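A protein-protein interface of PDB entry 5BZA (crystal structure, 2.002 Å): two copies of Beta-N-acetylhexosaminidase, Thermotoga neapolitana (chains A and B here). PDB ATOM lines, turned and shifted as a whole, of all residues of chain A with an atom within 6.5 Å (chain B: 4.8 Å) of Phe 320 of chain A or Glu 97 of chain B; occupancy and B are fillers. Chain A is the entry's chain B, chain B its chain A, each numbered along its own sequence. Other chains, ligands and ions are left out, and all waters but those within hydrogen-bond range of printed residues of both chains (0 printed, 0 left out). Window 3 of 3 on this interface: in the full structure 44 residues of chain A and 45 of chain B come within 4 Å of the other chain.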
ATOM      1  N   MET A  49      23.926  -4.320  34.547  1.00  0.00           N
ATOM      2  CA  MET A  49      23.063  -4.544  33.380  1.00  0.00           C
ATOM      3  C   MET A  49      23.659  -3.913  32.094  1.00  0.00           C
ATOM      4  O   MET A  49      23.622  -4.516  31.009  1.00  0.00           O
ATOM      5  CB  MET A  49      21.661  -3.984  33.617  1.00  0.00           C
ATOM      6  CG  MET A  49      20.903  -4.737  34.651  1.00  0.00           C
ATOM      7  SD  MET A  49      20.695  -6.537  34.376  1.00  0.00           S
ATOM      8  CE  MET A  49      19.772  -6.571  32.852  1.00  0.00           C
ATOM      9  N   MET A 103      10.252  -7.698  35.578  1.00  0.00           N
ATOM     10  CA  MET A 103      11.587  -8.289  35.493  1.00  0.00           C
ATOM     11  C   MET A 103      12.159  -8.178  34.088  1.00  0.00           C
ATOM     12  O   MET A 103      13.328  -7.777  33.884  1.00  0.00           O
ATOM     13  CB  MET A 103      11.555  -9.792  35.891  1.00  0.00           C
ATOM     14  CG  MET A 103      11.299 -10.086  37.345  1.00  0.00           C
ATOM     15  SD  MET A 103      10.853 -11.833  37.755  1.00  0.00           S
ATOM     16  CE  MET A 103      10.365 -11.593  39.473  1.00  0.00           C
ATOM     17  N   ASN A 104      11.328  -8.556  33.117  1.00  0.00           N
ATOM     18  CA  ASN A 104      11.712  -8.546  31.716  1.00  0.00           C
ATOM     19  C   ASN A 104      12.050  -7.112  31.323  1.00  0.00           C
ATOM     20  O   ASN A 104      12.991  -6.898  30.556  1.00  0.00           O
ATOM     21  CB  ASN A 104      10.601  -9.085  30.801  1.00  0.00           C
ATOM     22  CG  ASN A 104      10.970  -8.979  29.300  1.00  0.00           C
ATOM     23  OD1 ASN A 104      10.728  -7.958  28.640  1.00  0.00           O
ATOM     24  ND2 ASN A 104      11.554 -10.023  28.775  1.00  0.00           N
ATOM     25  N   THR A 105      11.271  -6.135  31.821  1.00  0.00           N
ATOM     26  CA  THR A 105      11.540  -4.729  31.492  1.00  0.00           C
ATOM     27  C   THR A 105      12.887  -4.323  32.047  1.00  0.00           C
ATOM     28  O   THR A 105      13.618  -3.551  31.420  1.00  0.00           O
ATOM     29  CB  THR A 105      10.457  -3.765  32.046  1.00  0.00           C
ATOM     30  OG1 THR A 105       9.175  -4.154  31.565  1.00  0.00           O
ATOM     31  CG2 THR A 105      10.719  -2.335  31.609  1.00  0.00           C
ATOM     32  N   LEU A 106      13.224  -4.810  33.244  1.00  0.00           N
ATOM     33  CA  LEU A 106      14.504  -4.414  33.826  1.00  0.00           C
ATOM     34  C   LEU A 106      15.705  -4.964  33.090  1.00  0.00           C
ATOM     35  O   LEU A 106      16.781  -4.364  33.137  1.00  0.00           O
ATOM     36  CB  LEU A 106      14.587  -4.816  35.284  1.00  0.00           C
ATOM     37  CG  LEU A 106      13.643  -4.144  36.272  1.00  0.00           C
ATOM     38  CD1 LEU A 106      13.761  -4.921  37.601  1.00  0.00           C
ATOM     39  CD2 LEU A 106      14.033  -2.658  36.432  1.00  0.00           C
ATOM     40  N   GLY A 107      15.513  -6.094  32.408  1.00  0.00           N
ATOM     41  CA  GLY A 107      16.580  -6.806  31.738  1.00  0.00           C
ATOM     42  C   GLY A 107      16.737  -8.264  32.202  1.00  0.00           C
ATOM     43  O   GLY A 107      17.595  -8.962  31.677  1.00  0.00           O
ATOM     44  N   PHE A 108      15.946  -8.739  33.166  1.00  0.00           N
ATOM     45  CA  PHE A 108      16.011 -10.176  33.530  1.00  0.00           C
ATOM     46  C   PHE A 108      15.359 -11.027  32.406  1.00  0.00           C
ATOM     47  O   PHE A 108      14.578 -10.504  31.619  1.00  0.00           O
ATOM     48  CB  PHE A 108      15.335 -10.419  34.890  1.00  0.00           C
ATOM     49  CG  PHE A 108      16.107  -9.852  36.059  1.00  0.00           C
ATOM     50  CD1 PHE A 108      17.104 -10.601  36.695  1.00  0.00           C
ATOM     51  CD2 PHE A 108      15.886  -8.518  36.474  1.00  0.00           C
ATOM     52  CE1 PHE A 108      17.833 -10.065  37.779  1.00  0.00           C
ATOM     53  CE2 PHE A 108      16.610  -7.953  37.536  1.00  0.00           C
ATOM     54  CZ  PHE A 108      17.589  -8.725  38.191  1.00  0.00           C
ATOM     55  N   ASN A 318      15.658 -10.032  23.668  1.00  0.00           N
ATOM     56  CA  ASN A 318      14.893  -8.985  24.370  1.00  0.00           C
ATOM     57  C   ASN A 318      15.296  -7.574  23.965  1.00  0.00           C
ATOM     58  O   ASN A 318      16.422  -7.349  23.538  1.00  0.00           O
ATOM     59  CB  ASN A 318      15.035  -9.142  25.894  1.00  0.00           C
ATOM     60  CG  ASN A 318      16.461  -8.834  26.398  1.00  0.00           C
ATOM     61  OD1 ASN A 318      17.438  -8.943  25.642  1.00  0.00           O
ATOM     62  ND2 ASN A 318      16.576  -8.413  27.664  1.00  0.00           N
ATOM     63  N   ARG A 319      14.350  -6.635  24.066  1.00  0.00           N
ATOM     64  CA  ARG A 319      14.606  -5.224  23.720  1.00  0.00           C
ATOM     65  C   ARG A 319      14.860  -4.344  24.943  1.00  0.00           C
ATOM     66  O   ARG A 319      15.274  -3.168  24.815  1.00  0.00           O
ATOM     67  CB  ARG A 319      13.455  -4.669  22.848  1.00  0.00           C
ATOM     68  CG  ARG A 319      12.103  -4.351  23.526  1.00  0.00           C
ATOM     69  CD  ARG A 319      11.068  -3.973  22.416  1.00  0.00           C
ATOM     70  NE  ARG A 319       9.689  -4.112  22.899  1.00  0.00           N
ATOM     71  CZ  ARG A 319       9.071  -5.294  23.031  1.00  0.00           C
ATOM     72  NH1 ARG A 319       9.750  -6.427  22.826  1.00  0.00           N
ATOM     73  NH2 ARG A 319       7.807  -5.359  23.457  1.00  0.00           N
ATOM     74  N   PHE A 320      14.636  -4.912  26.128  1.00  0.00           N
ATOM     75  CA  PHE A 320      14.730  -4.117  27.359  1.00  0.00           C
ATOM     76  C   PHE A 320      15.975  -4.388  28.204  1.00  0.00           C
ATOM     77  O   PHE A 320      16.280  -5.551  28.573  1.00  0.00           O
ATOM     78  CB  PHE A 320      13.468  -4.319  28.211  1.00  0.00           C
ATOM     79  CG  PHE A 320      12.214  -3.904  27.512  1.00  0.00           C
ATOM     80  CD1 PHE A 320      11.968  -2.557  27.254  1.00  0.00           C
ATOM     81  CD2 PHE A 320      11.286  -4.842  27.104  1.00  0.00           C
ATOM     82  CE1 PHE A 320      10.817  -2.155  26.606  1.00  0.00           C
ATOM     83  CE2 PHE A 320      10.128  -4.454  26.454  1.00  0.00           C
ATOM     84  CZ  PHE A 320       9.898  -3.103  26.200  1.00  0.00           C
ATOM     85  N   ASN A 321      16.679  -3.311  28.537  1.00  0.00           N
ATOM     86  CA  ASN A 321      17.770  -3.406  29.498  1.00  0.00           C
ATOM     87  C   ASN A 321      17.921  -2.069  30.265  1.00  0.00           C
ATOM     88  O   ASN A 321      18.315  -1.068  29.683  1.00  0.00           O
ATOM     89  CB  ASN A 321      19.069  -3.809  28.781  1.00  0.00           C
ATOM     90  CG  ASN A 321      20.174  -4.203  29.740  1.00  0.00           C
ATOM     91  OD1 ASN A 321      20.272  -3.667  30.811  1.00  0.00           O
ATOM     92  ND2 ASN A 321      21.024  -5.119  29.336  1.00  0.00           N
ATOM     93  N   SER A 322      17.594  -2.075  31.567  1.00  0.00           N
ATOM     94  CA  SER A 322      17.646  -0.885  32.416  1.00  0.00           C
ATOM     95  C   SER A 322      19.080  -0.292  32.538  1.00  0.00           C
ATOM     96  O   SER A 322      19.278   0.789  33.099  1.00  0.00           O
ATOM     97  CB  SER A 322      17.025  -1.193  33.785  1.00  0.00           C
ATOM     98  OG  SER A 322      17.732  -2.198  34.524  1.00  0.00           O
ATOM     99  N   LEU A 324      20.572   1.166  30.311  1.00  0.00           N
ATOM    100  CA  LEU A 324      20.542   2.405  29.560  1.00  0.00           C
ATOM    101  C   LEU A 324      20.715   3.569  30.537  1.00  0.00           C
ATOM    102  O   LEU A 324      21.330   4.603  30.207  1.00  0.00           O
ATOM    103  CB  LEU A 324      19.228   2.516  28.760  1.00  0.00           C
ATOM    104  CG  LEU A 324      17.942   2.699  29.567  1.00  0.00           C
ATOM    105  CD1 LEU A 324      17.531   4.210  29.765  1.00  0.00           C
ATOM    106  CD2 LEU A 324      16.809   1.837  28.986  1.00  0.00           C
ATOM    107  N   GLY B  93      13.845   8.290  25.187  1.00  0.00           N
ATOM    108  CA  GLY B  93      12.748   7.457  24.755  1.00  0.00           C
ATOM    109  C   GLY B  93      12.770   6.091  25.433  1.00  0.00           C
ATOM    110  O   GLY B  93      11.738   5.602  25.891  1.00  0.00           O
ATOM    111  N   ARG B  94      13.949   5.480  25.500  1.00  0.00           N
ATOM    112  CA  ARG B  94      14.084   4.140  26.086  1.00  0.00           C
ATOM    113  C   ARG B  94      13.758   4.202  27.545  1.00  0.00           C
ATOM    114  O   ARG B  94      13.066   3.307  28.059  1.00  0.00           O
ATOM    115  CB  ARG B  94      15.487   3.588  25.872  1.00  0.00           C
ATOM    116  CG  ARG B  94      15.837   3.467  24.424  1.00  0.00           C
ATOM    117  CD  ARG B  94      17.020   2.603  24.237  1.00  0.00           C
ATOM    118  NE  ARG B  94      17.406   2.513  22.834  1.00  0.00           N
ATOM    119  CZ  ARG B  94      18.672   2.464  22.413  1.00  0.00           C
ATOM    120  NH1 ARG B  94      19.680   2.496  23.301  1.00  0.00           N
ATOM    121  NH2 ARG B  94      18.922   2.366  21.106  1.00  0.00           N
ATOM    122  N   TYR B  95      14.227   5.272  28.209  1.00  0.00           N
ATOM    123  CA  TYR B  95      13.975   5.409  29.633  1.00  0.00           C
ATOM    124  C   TYR B  95      12.480   5.521  29.836  1.00  0.00           C
ATOM    125  O   TYR B  95      11.901   4.854  30.689  1.00  0.00           O
ATOM    126  CB  TYR B  95      14.721   6.604  30.276  1.00  0.00           C
ATOM    127  CG  TYR B  95      14.050   6.998  31.569  1.00  0.00           C
ATOM    128  CD1 TYR B  95      14.096   6.138  32.669  1.00  0.00           C
ATOM    129  CD2 TYR B  95      13.297   8.186  31.679  1.00  0.00           C
ATOM    130  CE1 TYR B  95      13.449   6.422  33.835  1.00  0.00           C
ATOM    131  CE2 TYR B  95      12.644   8.476  32.871  1.00  0.00           C
ATOM    132  CZ  TYR B  95      12.748   7.577  33.962  1.00  0.00           C
ATOM    133  OH  TYR B  95      12.124   7.801  35.184  1.00  0.00           O
ATOM    134  N   CYS B  96      11.822   6.345  29.041  1.00  0.00           N
ATOM    135  CA  CYS B  96      10.398   6.529  29.283  1.00  0.00           C
ATOM    136  C   CYS B  96       9.577   5.271  28.893  1.00  0.00           C
ATOM    137  O   CYS B  96       8.499   5.032  29.434  1.00  0.00           O
ATOM    138  CB  CYS B  96       9.886   7.762  28.530  1.00  0.00           C
ATOM    139  SG  CYS B  96      10.568   9.225  29.235  1.00  0.00           S
ATOM    140  N   GLU B  97      10.054   4.505  27.925  1.00  0.00           N
ATOM    141  CA  GLU B  97       9.357   3.265  27.588  1.00  0.00           C
ATOM    142  C   GLU B  97       9.452   2.272  28.766  1.00  0.00           C
ATOM    143  O   GLU B  97       8.455   1.701  29.174  1.00  0.00           O
ATOM    144  CB  GLU B  97       9.913   2.602  26.323  1.00  0.00           C
ATOM    145  CG  GLU B  97       9.019   1.426  25.913  1.00  0.00           C
ATOM    146  CD  GLU B  97       9.551   0.579  24.778  1.00  0.00           C
ATOM    147  OE1 GLU B  97      10.674   0.829  24.297  1.00  0.00           O
ATOM    148  OE2 GLU B  97       8.821  -0.336  24.350  1.00  0.00           O
ATOM    149  N   MET B  98      10.656   2.117  29.307  1.00  0.00           N
ATOM    150  CA  MET B  98      10.879   1.277  30.487  1.00  0.00           C
ATOM    151  C   MET B  98       9.987   1.693  31.645  1.00  0.00           C
ATOM    152  O   MET B  98       9.304   0.837  32.287  1.00  0.00           O
ATOM    153  CB  MET B  98      12.330   1.352  30.912  1.00  0.00           C
ATOM    154  CG  MET B  98      12.679   0.495  32.125  1.00  0.00           C
ATOM    155  SD  MET B  98      14.071   1.209  33.042  1.00  0.00           S
ATOM    156  CE  MET B  98      13.254   2.572  33.893  1.00  0.00           C
ATOM    157  N   ALA B  99      10.030   3.002  31.935  1.00  0.00           N
ATOM    158  CA  ALA B  99       9.290   3.557  33.068  1.00  0.00           C
ATOM    159  C   ALA B  99       7.811   3.346  32.843  1.00  0.00           C
ATOM    160  O   ALA B  99       7.077   2.889  33.736  1.00  0.00           O
ATOM    161  CB  ALA B  99       9.625   5.055  33.280  1.00  0.00           C
ATOM    162  N   GLY B 100       7.369   3.634  31.625  1.00  0.00           N
ATOM    163  CA  GLY B 100       5.953   3.517  31.297  1.00  0.00           C
ATOM    164  C   GLY B 100       5.480   2.078  31.366  1.00  0.00           C
ATOM    165  O   GLY B 100       4.370   1.787  31.786  1.00  0.00           O
ATOM    166  N   ARG B 101       6.324   1.161  30.935  1.00  0.00           N
ATOM    167  CA  ARG B 101       5.949  -0.259  30.901  1.00  0.00           C
ATOM    168  C   ARG B 101       5.702  -0.737  32.327  1.00  0.00           C
ATOM    169  O   ARG B 101       4.656  -1.348  32.637  1.00  0.00           O
ATOM    170  CB  ARG B 101       7.039  -1.059  30.199  1.00  0.00           C
ATOM    171  CG  ARG B 101       6.546  -2.352  29.660  1.00  0.00           C
ATOM    172  CD  ARG B 101       7.492  -2.911  28.641  1.00  0.00           C
ATOM    173  NE  ARG B 101       6.865  -4.080  28.029  1.00  0.00           N
ATOM    174  CZ  ARG B 101       7.229  -5.332  28.274  1.00  0.00           C
ATOM    175  NH1 ARG B 101       8.247  -5.595  29.104  1.00  0.00           N
ATOM    176  NH2 ARG B 101       6.573  -6.320  27.677  1.00  0.00           N
ATOM    177  N   GLY B 149       7.923   7.305  23.988  1.00  0.00           N
ATOM    178  CA  GLY B 149       8.376   6.228  24.857  1.00  0.00           C
ATOM    179  C   GLY B 149       7.352   5.894  25.935  1.00  0.00           C
ATOM    180  O   GLY B 149       7.002   4.728  26.126  1.00  0.00           O
ATOM    181  N   TYR B 150       6.937   6.903  26.691  1.00  0.00           N
ATOM    182  CA  TYR B 150       5.893   6.707  27.681  1.00  0.00           C
ATOM    183  C   TYR B 150       4.706   6.024  27.075  1.00  0.00           C
ATOM    184  O   TYR B 150       4.172   5.059  27.638  1.00  0.00           O
ATOM    185  CB  TYR B 150       5.439   8.025  28.273  1.00  0.00           C
ATOM    186  CG  TYR B 150       6.308   8.553  29.381  1.00  0.00           C
ATOM    187  CD1 TYR B 150       6.762   7.708  30.416  1.00  0.00           C
ATOM    188  CD2 TYR B 150       6.651   9.910  29.423  1.00  0.00           C
ATOM    189  CE1 TYR B 150       7.559   8.206  31.449  1.00  0.00           C
ATOM    190  CE2 TYR B 150       7.433  10.410  30.432  1.00  0.00           C
ATOM    191  CZ  TYR B 150       7.878   9.586  31.445  1.00  0.00           C
ATOM    192  OH  TYR B 150       8.667  10.159  32.437  1.00  0.00           O
ATOM    193  N   LYS B 152       4.408   4.198  24.224  1.00  0.00           N
ATOM    194  CA  LYS B 152       4.795   2.851  23.809  1.00  0.00           C
ATOM    195  C   LYS B 152       4.790   1.879  25.011  1.00  0.00           C
ATOM    196  O   LYS B 152       4.429   0.713  24.898  1.00  0.00           O
ATOM    197  CB  LYS B 152       6.181   2.916  23.147  1.00  0.00           C
ATOM    198  CG  LYS B 152       6.653   1.687  22.363  1.00  0.00           C
ATOM    199  CD  LYS B 152       8.094   1.926  21.923  1.00  0.00           C
ATOM    200  CE  LYS B 152       8.674   0.766  21.096  1.00  0.00           C
ATOM    201  NZ  LYS B 152       7.979   0.677  19.787  1.00  0.00           N
ATOM    202  N   GLY B 153       5.243   2.383  26.149  1.00  0.00           N
ATOM    203  CA  GLY B 153       5.268   1.646  27.396  1.00  0.00           C
ATOM    204  C   GLY B 153       3.892   1.354  27.975  1.00  0.00           C
ATOM    205  O   GLY B 153       3.754   0.410  28.736  1.00  0.00           O
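The guanidinium group (NH1) of Arg 101 of chain B is in hydrogen-bond range of the side-chain amide oxygen (OD1) of Asn 104 of chain A (3.5 Å).
OG1 of Thr 105 of chain A sits at hydrogen-bond distance from NH1 of Arg 101 of chain B (3.0 Å).
The side-chain amide nitrogen (ND2) of Asn 318 of chain A lies within hydrogen-bond range of the backbone carbonyl oxygen (O) of Phe 320 of chain A.
The backbone NH (N) of Arg 101 of chain B lies close to the backbone carbonyl oxygen (O) of Gly 153 of chain B, at 3.5 Å.
O of Leu 106 of chain A sits at hydrogen-bond distance from OG of Ser 322 of chain A (2.7 Å).
Among the printed residues, pairs that only touch across the chains: Phe 320 of chain A with Arg 101 of chain B (3.4 Å), Thr 105 of chain A with Met 98 of chain B (3.5 Å), Phe 320 of chain A with Glu 97 of chain B (3.5 Å), Leu 324 of chain A with Tyr 95 of chain B (3.7 Å), Leu 324 of chain A with Arg 94 of chain B (3.8 Å) and Ser 322 of chain A with Met 98 of chain B (3.9 Å).
Printed residues of chain B within 4 Å of Asn 104 of chain A: Arg 101.
Leu 106 of chain A touches none of the printed residues of chain B.
Printed residues of chain B within 4 Å of Phe 320 of chain A: Glu 97 and Arg 101.
Of the printed residues of chain B, Ser 322 of chain A touches Met 98.
Of the printed residues of chain A, Arg 94 of chain B touches Leu 324 (3.8 Å).
Glu 97 of chain B touches one residue of chain A.
The nearest residue of chain A that does not touch Glu 97 of chain B is Arg 319 of chain A (4.1 Å).
Printed residues of chain B that touch a printed residue of chain A: Arg 94, Tyr 95, Glu 97, Met 98 and Arg 101.
Hydrophobic or aromatic side chains of chain B within 4 Å of the printed part of chain A: Tyr 95 and Met 98.
Along chain A the printed residues that touch a printed residue of chain B span positions 104 to 324.
Among the printed residues, no Asp or Glu carboxylate lies within 4 Å of a Lys or Arg side-chain nitrogen of the other chain.
No position is printed for both chains.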
